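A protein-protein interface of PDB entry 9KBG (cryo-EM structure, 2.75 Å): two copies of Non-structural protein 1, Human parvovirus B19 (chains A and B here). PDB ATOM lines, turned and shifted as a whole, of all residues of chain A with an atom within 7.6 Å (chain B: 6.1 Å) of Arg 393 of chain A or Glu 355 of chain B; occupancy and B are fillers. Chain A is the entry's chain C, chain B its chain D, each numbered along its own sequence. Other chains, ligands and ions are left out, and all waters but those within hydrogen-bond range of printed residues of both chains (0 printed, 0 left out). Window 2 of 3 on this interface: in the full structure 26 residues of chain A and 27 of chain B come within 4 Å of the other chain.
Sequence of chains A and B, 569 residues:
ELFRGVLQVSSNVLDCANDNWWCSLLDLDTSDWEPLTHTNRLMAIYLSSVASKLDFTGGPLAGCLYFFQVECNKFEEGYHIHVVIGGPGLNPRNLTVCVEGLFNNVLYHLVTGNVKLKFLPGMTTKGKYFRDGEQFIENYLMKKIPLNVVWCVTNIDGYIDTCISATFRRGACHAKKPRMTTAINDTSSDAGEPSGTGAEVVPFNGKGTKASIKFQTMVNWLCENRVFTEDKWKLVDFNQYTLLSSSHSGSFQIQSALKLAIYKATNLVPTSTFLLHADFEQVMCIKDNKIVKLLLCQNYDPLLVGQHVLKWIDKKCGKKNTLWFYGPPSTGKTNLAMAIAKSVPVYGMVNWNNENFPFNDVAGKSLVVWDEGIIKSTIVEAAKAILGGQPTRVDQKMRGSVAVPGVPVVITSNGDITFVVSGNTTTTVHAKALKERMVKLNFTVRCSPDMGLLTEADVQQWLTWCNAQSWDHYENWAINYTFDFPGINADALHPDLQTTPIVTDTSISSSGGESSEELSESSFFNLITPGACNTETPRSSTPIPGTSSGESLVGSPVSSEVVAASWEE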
ATOM      1  N   GLN A 390       2.605   6.954 -22.595  1.00  0.00           N
ATOM      2  CA  GLN A 390       3.296   7.968 -23.379  1.00  0.00           C
ATOM      3  C   GLN A 390       4.368   8.655 -22.536  1.00  0.00           C
ATOM      4  O   GLN A 390       4.139   8.951 -21.360  1.00  0.00           O
ATOM      5  CB  GLN A 390       2.308   9.008 -23.904  1.00  0.00           C
ATOM      6  CG  GLN A 390       1.475   8.539 -25.085  1.00  0.00           C
ATOM      7  CD  GLN A 390       0.136   7.966 -24.665  1.00  0.00           C
ATOM      8  OE1 GLN A 390      -0.745   8.694 -24.206  1.00  0.00           O
ATOM      9  NE2 GLN A 390      -0.025   6.658 -24.822  1.00  0.00           N
ATOM     10  N   PRO A 391       5.540   8.915 -23.106  1.00  0.00           N
ATOM     11  CA  PRO A 391       6.559   9.687 -22.388  1.00  0.00           C
ATOM     12  C   PRO A 391       6.143  11.144 -22.244  1.00  0.00           C
ATOM     13  O   PRO A 391       5.188  11.619 -22.860  1.00  0.00           O
ATOM     14  CB  PRO A 391       7.806   9.550 -23.267  1.00  0.00           C
ATOM     15  CG  PRO A 391       7.289   9.162 -24.612  1.00  0.00           C
ATOM     16  CD  PRO A 391       6.049   8.365 -24.373  1.00  0.00           C
ATOM     17  N   THR A 392       6.888  11.857 -21.409  1.00  0.00           N
ATOM     18  CA  THR A 392       6.648  13.271 -21.170  1.00  0.00           C
ATOM     19  C   THR A 392       7.555  14.120 -22.053  1.00  0.00           C
ATOM     20  O   THR A 392       8.555  13.646 -22.597  1.00  0.00           O
ATOM     21  CB  THR A 392       6.869  13.625 -19.696  1.00  0.00           C
ATOM     22  OG1 THR A 392       6.490  14.987 -19.465  1.00  0.00           O
ATOM     23  CG2 THR A 392       8.329  13.440 -19.314  1.00  0.00           C
ATOM     24  N   ARG A 393       7.180  15.394 -22.195  1.00  0.00           N
ATOM     25  CA  ARG A 393       7.935  16.306 -23.049  1.00  0.00           C
ATOM     26  C   ARG A 393       9.377  16.448 -22.577  1.00  0.00           C
ATOM     27  O   ARG A 393      10.301  16.541 -23.393  1.00  0.00           O
ATOM     28  CB  ARG A 393       7.246  17.671 -23.089  1.00  0.00           C
ATOM     29  CG  ARG A 393       5.852  17.643 -23.698  1.00  0.00           C
ATOM     30  CD  ARG A 393       5.026  18.836 -23.245  1.00  0.00           C
ATOM     31  NE  ARG A 393       5.496  20.089 -23.822  1.00  0.00           N
ATOM     32  CZ  ARG A 393       4.956  20.676 -24.881  1.00  0.00           C
ATOM     33  NH1 ARG A 393       3.918  20.149 -25.508  1.00  0.00           N
ATOM     34  NH2 ARG A 393       5.470  21.822 -25.320  1.00  0.00           N
ATOM     35  N   VAL A 394       9.587  16.469 -21.259  1.00  0.00           N
ATOM     36  CA  VAL A 394      10.939  16.587 -20.721  1.00  0.00           C
ATOM     37  C   VAL A 394      11.777  15.371 -21.099  1.00  0.00           C
ATOM     38  O   VAL A 394      12.934  15.503 -21.515  1.00  0.00           O
ATOM     39  CB  VAL A 394      10.888  16.790 -19.196  1.00  0.00           C
ATOM     40  CG1 VAL A 394      12.267  16.600 -18.584  1.00  0.00           C
ATOM     41  CG2 VAL A 394      10.335  18.167 -18.864  1.00  0.00           C
ATOM     42  N   ASP A 395      11.209  14.170 -20.962  1.00  0.00           N
ATOM     43  CA  ASP A 395      11.943  12.959 -21.315  1.00  0.00           C
ATOM     44  C   ASP A 395      12.248  12.912 -22.807  1.00  0.00           C
ATOM     45  O   ASP A 395      13.346  12.512 -23.212  1.00  0.00           O
ATOM     46  CB  ASP A 395      11.151  11.724 -20.888  1.00  0.00           C
ATOM     47  CG  ASP A 395      11.954  10.446 -21.013  1.00  0.00           C
ATOM     48  OD1 ASP A 395      12.786  10.174 -20.121  1.00  0.00           O
ATOM     49  OD2 ASP A 395      11.755   9.713 -22.003  1.00  0.00           O
ATOM     50  N   GLN A 396      11.283  13.309 -23.640  1.00  0.00           N
ATOM     51  CA  GLN A 396      11.501  13.313 -25.084  1.00  0.00           C
ATOM     52  C   GLN A 396      12.583  14.311 -25.479  1.00  0.00           C
ATOM     53  O   GLN A 396      13.435  14.010 -26.323  1.00  0.00           O
ATOM     54  CB  GLN A 396      10.191  13.627 -25.807  1.00  0.00           C
ATOM     55  CG  GLN A 396       9.146  12.530 -25.701  1.00  0.00           C
ATOM     56  CD  GLN A 396       7.976  12.746 -26.640  1.00  0.00           C
ATOM     57  OE1 GLN A 396       8.037  13.576 -27.546  1.00  0.00           O
ATOM     58  NE2 GLN A 396       6.901  11.996 -26.427  1.00  0.00           N
ATOM     59  N   LYS A 397      12.560  15.506 -24.885  1.00  0.00           N
ATOM     60  CA  LYS A 397      13.553  16.523 -25.213  1.00  0.00           C
ATOM     61  C   LYS A 397      14.949  16.107 -24.766  1.00  0.00           C
ATOM     62  O   LYS A 397      15.930  16.338 -25.482  1.00  0.00           O
ATOM     63  CB  LYS A 397      13.158  17.855 -24.576  1.00  0.00           C
ATOM     64  CG  LYS A 397      14.065  19.020 -24.931  1.00  0.00           C
ATOM     65  CD  LYS A 397      13.449  20.337 -24.490  1.00  0.00           C
ATOM     66  CE  LYS A 397      13.963  21.498 -25.322  1.00  0.00           C
ATOM     67  NZ  LYS A 397      13.515  22.810 -24.780  1.00  0.00           N
ATOM     68  N   MET A 398      15.058  15.499 -23.583  1.00  0.00           N
ATOM     69  CA  MET A 398      16.368  15.160 -23.035  1.00  0.00           C
ATOM     70  C   MET A 398      17.062  14.088 -23.867  1.00  0.00           C
ATOM     71  O   MET A 398      18.253  14.204 -24.178  1.00  0.00           O
ATOM     72  CB  MET A 398      16.221  14.705 -21.583  1.00  0.00           C
ATOM     73  CG  MET A 398      17.490  14.128 -20.977  1.00  0.00           C
ATOM     74  SD  MET A 398      18.895  15.251 -21.107  1.00  0.00           S
ATOM     75  CE  MET A 398      20.064  14.457 -20.005  1.00  0.00           C
ATOM     76  N   ARG A 399      16.334  13.035 -24.239  1.00  0.00           N
ATOM     77  CA  ARG A 399      16.931  11.924 -24.968  1.00  0.00           C
ATOM     78  C   ARG A 399      16.929  12.121 -26.478  1.00  0.00           C
ATOM     79  O   ARG A 399      17.543  11.317 -27.189  1.00  0.00           O
ATOM     80  CB  ARG A 399      16.205  10.621 -24.622  1.00  0.00           C
ATOM     81  N   SER A 401      14.439  11.800 -28.691  1.00  0.00           N
ATOM     82  CA  SER A 401      13.653  10.801 -29.402  1.00  0.00           C
ATOM     83  C   SER A 401      12.225  10.847 -28.880  1.00  0.00           C
ATOM     84  O   SER A 401      11.944  11.443 -27.837  1.00  0.00           O
ATOM     85  CB  SER A 401      14.255   9.399 -29.256  1.00  0.00           C
ATOM     86  OG  SER A 401      14.484   9.074 -27.899  1.00  0.00           O
ATOM     87  N   VAL B 350       9.467  21.006 -32.623  1.00  0.00           N
ATOM     88  CA  VAL B 350       8.846  22.209 -32.083  1.00  0.00           C
ATOM     89  C   VAL B 350       7.863  21.868 -30.970  1.00  0.00           C
ATOM     90  O   VAL B 350       7.605  22.701 -30.094  1.00  0.00           O
ATOM     91  CB  VAL B 350       8.150  23.000 -33.207  1.00  0.00           C
ATOM     92  CG1 VAL B 350       7.715  24.370 -32.718  1.00  0.00           C
ATOM     93  CG2 VAL B 350       9.069  23.132 -34.407  1.00  0.00           C
ATOM     94  N   ASN B 351       7.318  20.650 -30.974  1.00  0.00           N
ATOM     95  CA  ASN B 351       6.348  20.250 -29.964  1.00  0.00           C
ATOM     96  C   ASN B 351       6.983  20.054 -28.594  1.00  0.00           C
ATOM     97  O   ASN B 351       6.332  20.308 -27.575  1.00  0.00           O
ATOM     98  CB  ASN B 351       5.643  18.965 -30.400  1.00  0.00           C
ATOM     99  CG  ASN B 351       5.211  19.002 -31.852  1.00  0.00           C
ATOM    100  OD1 ASN B 351       6.038  18.925 -32.759  1.00  0.00           O
ATOM    101  ND2 ASN B 351       3.909  19.119 -32.078  1.00  0.00           N
ATOM    102  N   TRP B 352       8.239  19.600 -28.546  1.00  0.00           N
ATOM    103  CA  TRP B 352       8.899  19.378 -27.262  1.00  0.00           C
ATOM    104  C   TRP B 352       9.135  20.689 -26.523  1.00  0.00           C
ATOM    105  O   TRP B 352       9.061  20.733 -25.290  1.00  0.00           O
ATOM    106  CB  TRP B 352      10.225  18.647 -27.468  1.00  0.00           C
ATOM    107  CG  TRP B 352      10.083  17.279 -28.047  1.00  0.00           C
ATOM    108  CD1 TRP B 352       8.973  16.487 -28.021  1.00  0.00           C
ATOM    109  CD2 TRP B 352      11.092  16.534 -28.739  1.00  0.00           C
ATOM    110  NE1 TRP B 352       9.227  15.296 -28.657  1.00  0.00           N
ATOM    111  CE2 TRP B 352      10.520  15.299 -29.106  1.00  0.00           C
ATOM    112  CE3 TRP B 352      12.421  16.791 -29.086  1.00  0.00           C
ATOM    113  CZ2 TRP B 352      11.233  14.325 -29.801  1.00  0.00           C
ATOM    114  CZ3 TRP B 352      13.126  15.823 -29.776  1.00  0.00           C
ATOM    115  CH2 TRP B 352      12.530  14.606 -30.126  1.00  0.00           C
ATOM    116  N   ASN B 353       9.424  21.759 -27.257  1.00  0.00           N
ATOM    117  CA  ASN B 353       9.789  23.028 -26.647  1.00  0.00           C
ATOM    118  C   ASN B 353       8.597  23.643 -25.913  1.00  0.00           C
ATOM    119  O   ASN B 353       7.450  23.209 -26.049  1.00  0.00           O
ATOM    120  CB  ASN B 353      10.316  23.993 -27.707  1.00  0.00           C
ATOM    121  CG  ASN B 353      11.500  23.430 -28.467  1.00  0.00           C
ATOM    122  OD1 ASN B 353      12.041  22.385 -28.110  1.00  0.00           O
ATOM    123  ND2 ASN B 353      11.906  24.122 -29.526  1.00  0.00           N
ATOM    124  N   ASN B 354       8.891  24.671 -25.121  1.00  0.00           N
ATOM    125  CA  ASN B 354       7.857  25.367 -24.371  1.00  0.00           C
ATOM    126  C   ASN B 354       6.906  26.094 -25.315  1.00  0.00           C
ATOM    127  O   ASN B 354       7.285  26.524 -26.407  1.00  0.00           O
ATOM    128  CB  ASN B 354       8.488  26.360 -23.394  1.00  0.00           C
ATOM    129  CG  ASN B 354       7.519  26.820 -22.321  1.00  0.00           C
ATOM    130  OD1 ASN B 354       6.463  26.221 -22.123  1.00  0.00           O
ATOM    131  ND2 ASN B 354       7.877  27.890 -21.622  1.00  0.00           N
ATOM    132  N   GLU B 355       5.650  26.226 -24.879  1.00  0.00           N
ATOM    133  CA  GLU B 355       4.636  26.866 -25.711  1.00  0.00           C
ATOM    134  C   GLU B 355       4.944  28.333 -25.978  1.00  0.00           C
ATOM    135  O   GLU B 355       4.497  28.873 -26.995  1.00  0.00           O
ATOM    136  CB  GLU B 355       3.258  26.735 -25.059  1.00  0.00           C
ATOM    137  CG  GLU B 355       2.726  25.310 -24.994  1.00  0.00           C
ATOM    138  CD  GLU B 355       3.272  24.530 -23.812  1.00  0.00           C
ATOM    139  OE1 GLU B 355       4.018  25.117 -23.003  1.00  0.00           O
ATOM    140  OE2 GLU B 355       2.953  23.329 -23.694  1.00  0.00           O
ATOM    141  N   ASN B 356       5.695  28.991 -25.094  1.00  0.00           N
ATOM    142  CA  ASN B 356       6.073  30.382 -25.299  1.00  0.00           C
ATOM    143  C   ASN B 356       7.414  30.542 -26.000  1.00  0.00           C
ATOM    144  O   ASN B 356       7.669  31.605 -26.576  1.00  0.00           O
ATOM    145  CB  ASN B 356       6.117  31.124 -23.958  1.00  0.00           C
ATOM    146  CG  ASN B 356       4.881  30.878 -23.115  1.00  0.00           C
ATOM    147  OD1 ASN B 356       4.906  30.085 -22.174  1.00  0.00           O
ATOM    148  ND2 ASN B 356       3.791  31.556 -23.452  1.00  0.00           N
ATOM    149  N   PHE B 357       8.268  29.521 -25.968  1.00  0.00           N
ATOM    150  CA  PHE B 357       9.568  29.543 -26.639  1.00  0.00           C
ATOM    151  C   PHE B 357       9.683  28.278 -27.478  1.00  0.00           C
ATOM    152  O   PHE B 357      10.254  27.273 -27.034  1.00  0.00           O
ATOM    153  CB  PHE B 357      10.710  29.653 -25.632  1.00  0.00           C
ATOM    154  CG  PHE B 357      10.486  30.694 -24.574  1.00  0.00           C
ATOM    155  CD1 PHE B 357      10.733  32.031 -24.836  1.00  0.00           C
ATOM    156  CD2 PHE B 357      10.025  30.337 -23.318  1.00  0.00           C
ATOM    157  CE1 PHE B 357      10.526  32.993 -23.865  1.00  0.00           C
ATOM    158  CE2 PHE B 357       9.817  31.294 -22.343  1.00  0.00           C
ATOM    159  CZ  PHE B 357      10.067  32.623 -22.617  1.00  0.00           C
ATOM    160  N   PRO B 358       9.145  28.288 -28.701  1.00  0.00           N
ATOM    161  CA  PRO B 358       9.159  27.072 -29.524  1.00  0.00           C
ATOM    162  C   PRO B 358      10.442  26.858 -30.309  1.00  0.00           C
ATOM    163  O   PRO B 358      10.570  25.820 -30.972  1.00  0.00           O
ATOM    164  CB  PRO B 358       7.972  27.287 -30.470  1.00  0.00           C
ATOM    165  CG  PRO B 358       7.895  28.774 -30.626  1.00  0.00           C
ATOM    166  CD  PRO B 358       8.440  29.400 -29.362  1.00  0.00           C
ATOM    167  N   ILE B 379       4.242  35.106 -32.118  1.00  0.00           N
ATOM    168  CA  ILE B 379       5.516  34.519 -32.514  1.00  0.00           C
ATOM    169  C   ILE B 379       5.730  34.616 -34.023  1.00  0.00           C
ATOM    170  O   ILE B 379       6.560  33.899 -34.577  1.00  0.00           O
ATOM    171  CB  ILE B 379       5.635  33.066 -32.026  1.00  0.00           C
ATOM    172  CG1 ILE B 379       4.613  32.177 -32.739  1.00  0.00           C
ATOM    173  CG2 ILE B 379       5.454  32.990 -30.521  1.00  0.00           C
ATOM    174  CD1 ILE B 379       4.845  30.697 -32.537  1.00  0.00           C
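NH2 of Arg 393 of chain A is in hydrogen-bond range of O of Asn 351 of chain B, 2.8 Å away. The guanidinium group (NH2) of Arg 393 of chain A lies within hydrogen-bond range of the backbone carbonyl oxygen (O) of Asn 353 of chain B (2.5 Å). OE2 of Glu 355 of chain B is in salt-bridge range of NH2 of Arg 393 of chain A (3.4 Å). OE1 of Gln 396 of chain A sits close to NE1 of Trp 352 of chain B (2.4 Å).
O of Trp 352 of chain B touches NH2 of Arg 393 of chain A, 3.8 Å away. Lys 397 of chain A touches Asn 353 of chain B (CE to OD1, 3.5 Å). O of Ser 401 of chain A touches CZ2 of Trp 352 of chain B (3.6 Å).
Arg 393 of chain A touches just these residues of chain B: Asn 351, Trp 352, Asn 353 and Glu 355. Of the printed residues of chain B, Gln 396 of chain A touches Trp 352. Printed residues of chain B within 4 Å of Ser 401 of chain A: Trp 352. The nearest printed residue of chain B that does not touch Lys 397 of chain A is Trp 352 of chain B (4.04 Å).
Hydrophobic or aromatic side chains of chain B within 4 Å of the printed part of chain A: Trp 352. Of the 11 printed residues of chain A, 4 touch a printed residue of chain B. Along chain A the printed residues that touch a printed residue of chain B span positions 393 to 401. Among the printed residues, Asp or Glu carboxylates within 4 Å of a Lys or Arg side-chain nitrogen of the other chain: Arg 393 of chain A with Glu 355 of chain B.
No position is printed for both chains.
The backbone carbonyl oxygen (O) of Gln 396 of chain A is in hydrogen-bond range of the backbone NH (N) of Ser 401 of chain A. The backbone carbonyl oxygen (O) of Pro 358 of chain B sits at hydrogen-bond distance from the side-chain amide nitrogen (ND2) of Asn 353 of chain B, 2.6 Å away. OE1 of Glu 355 of chain B lies close to OD1 of Asn 354 of chain B (2.8 Å).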
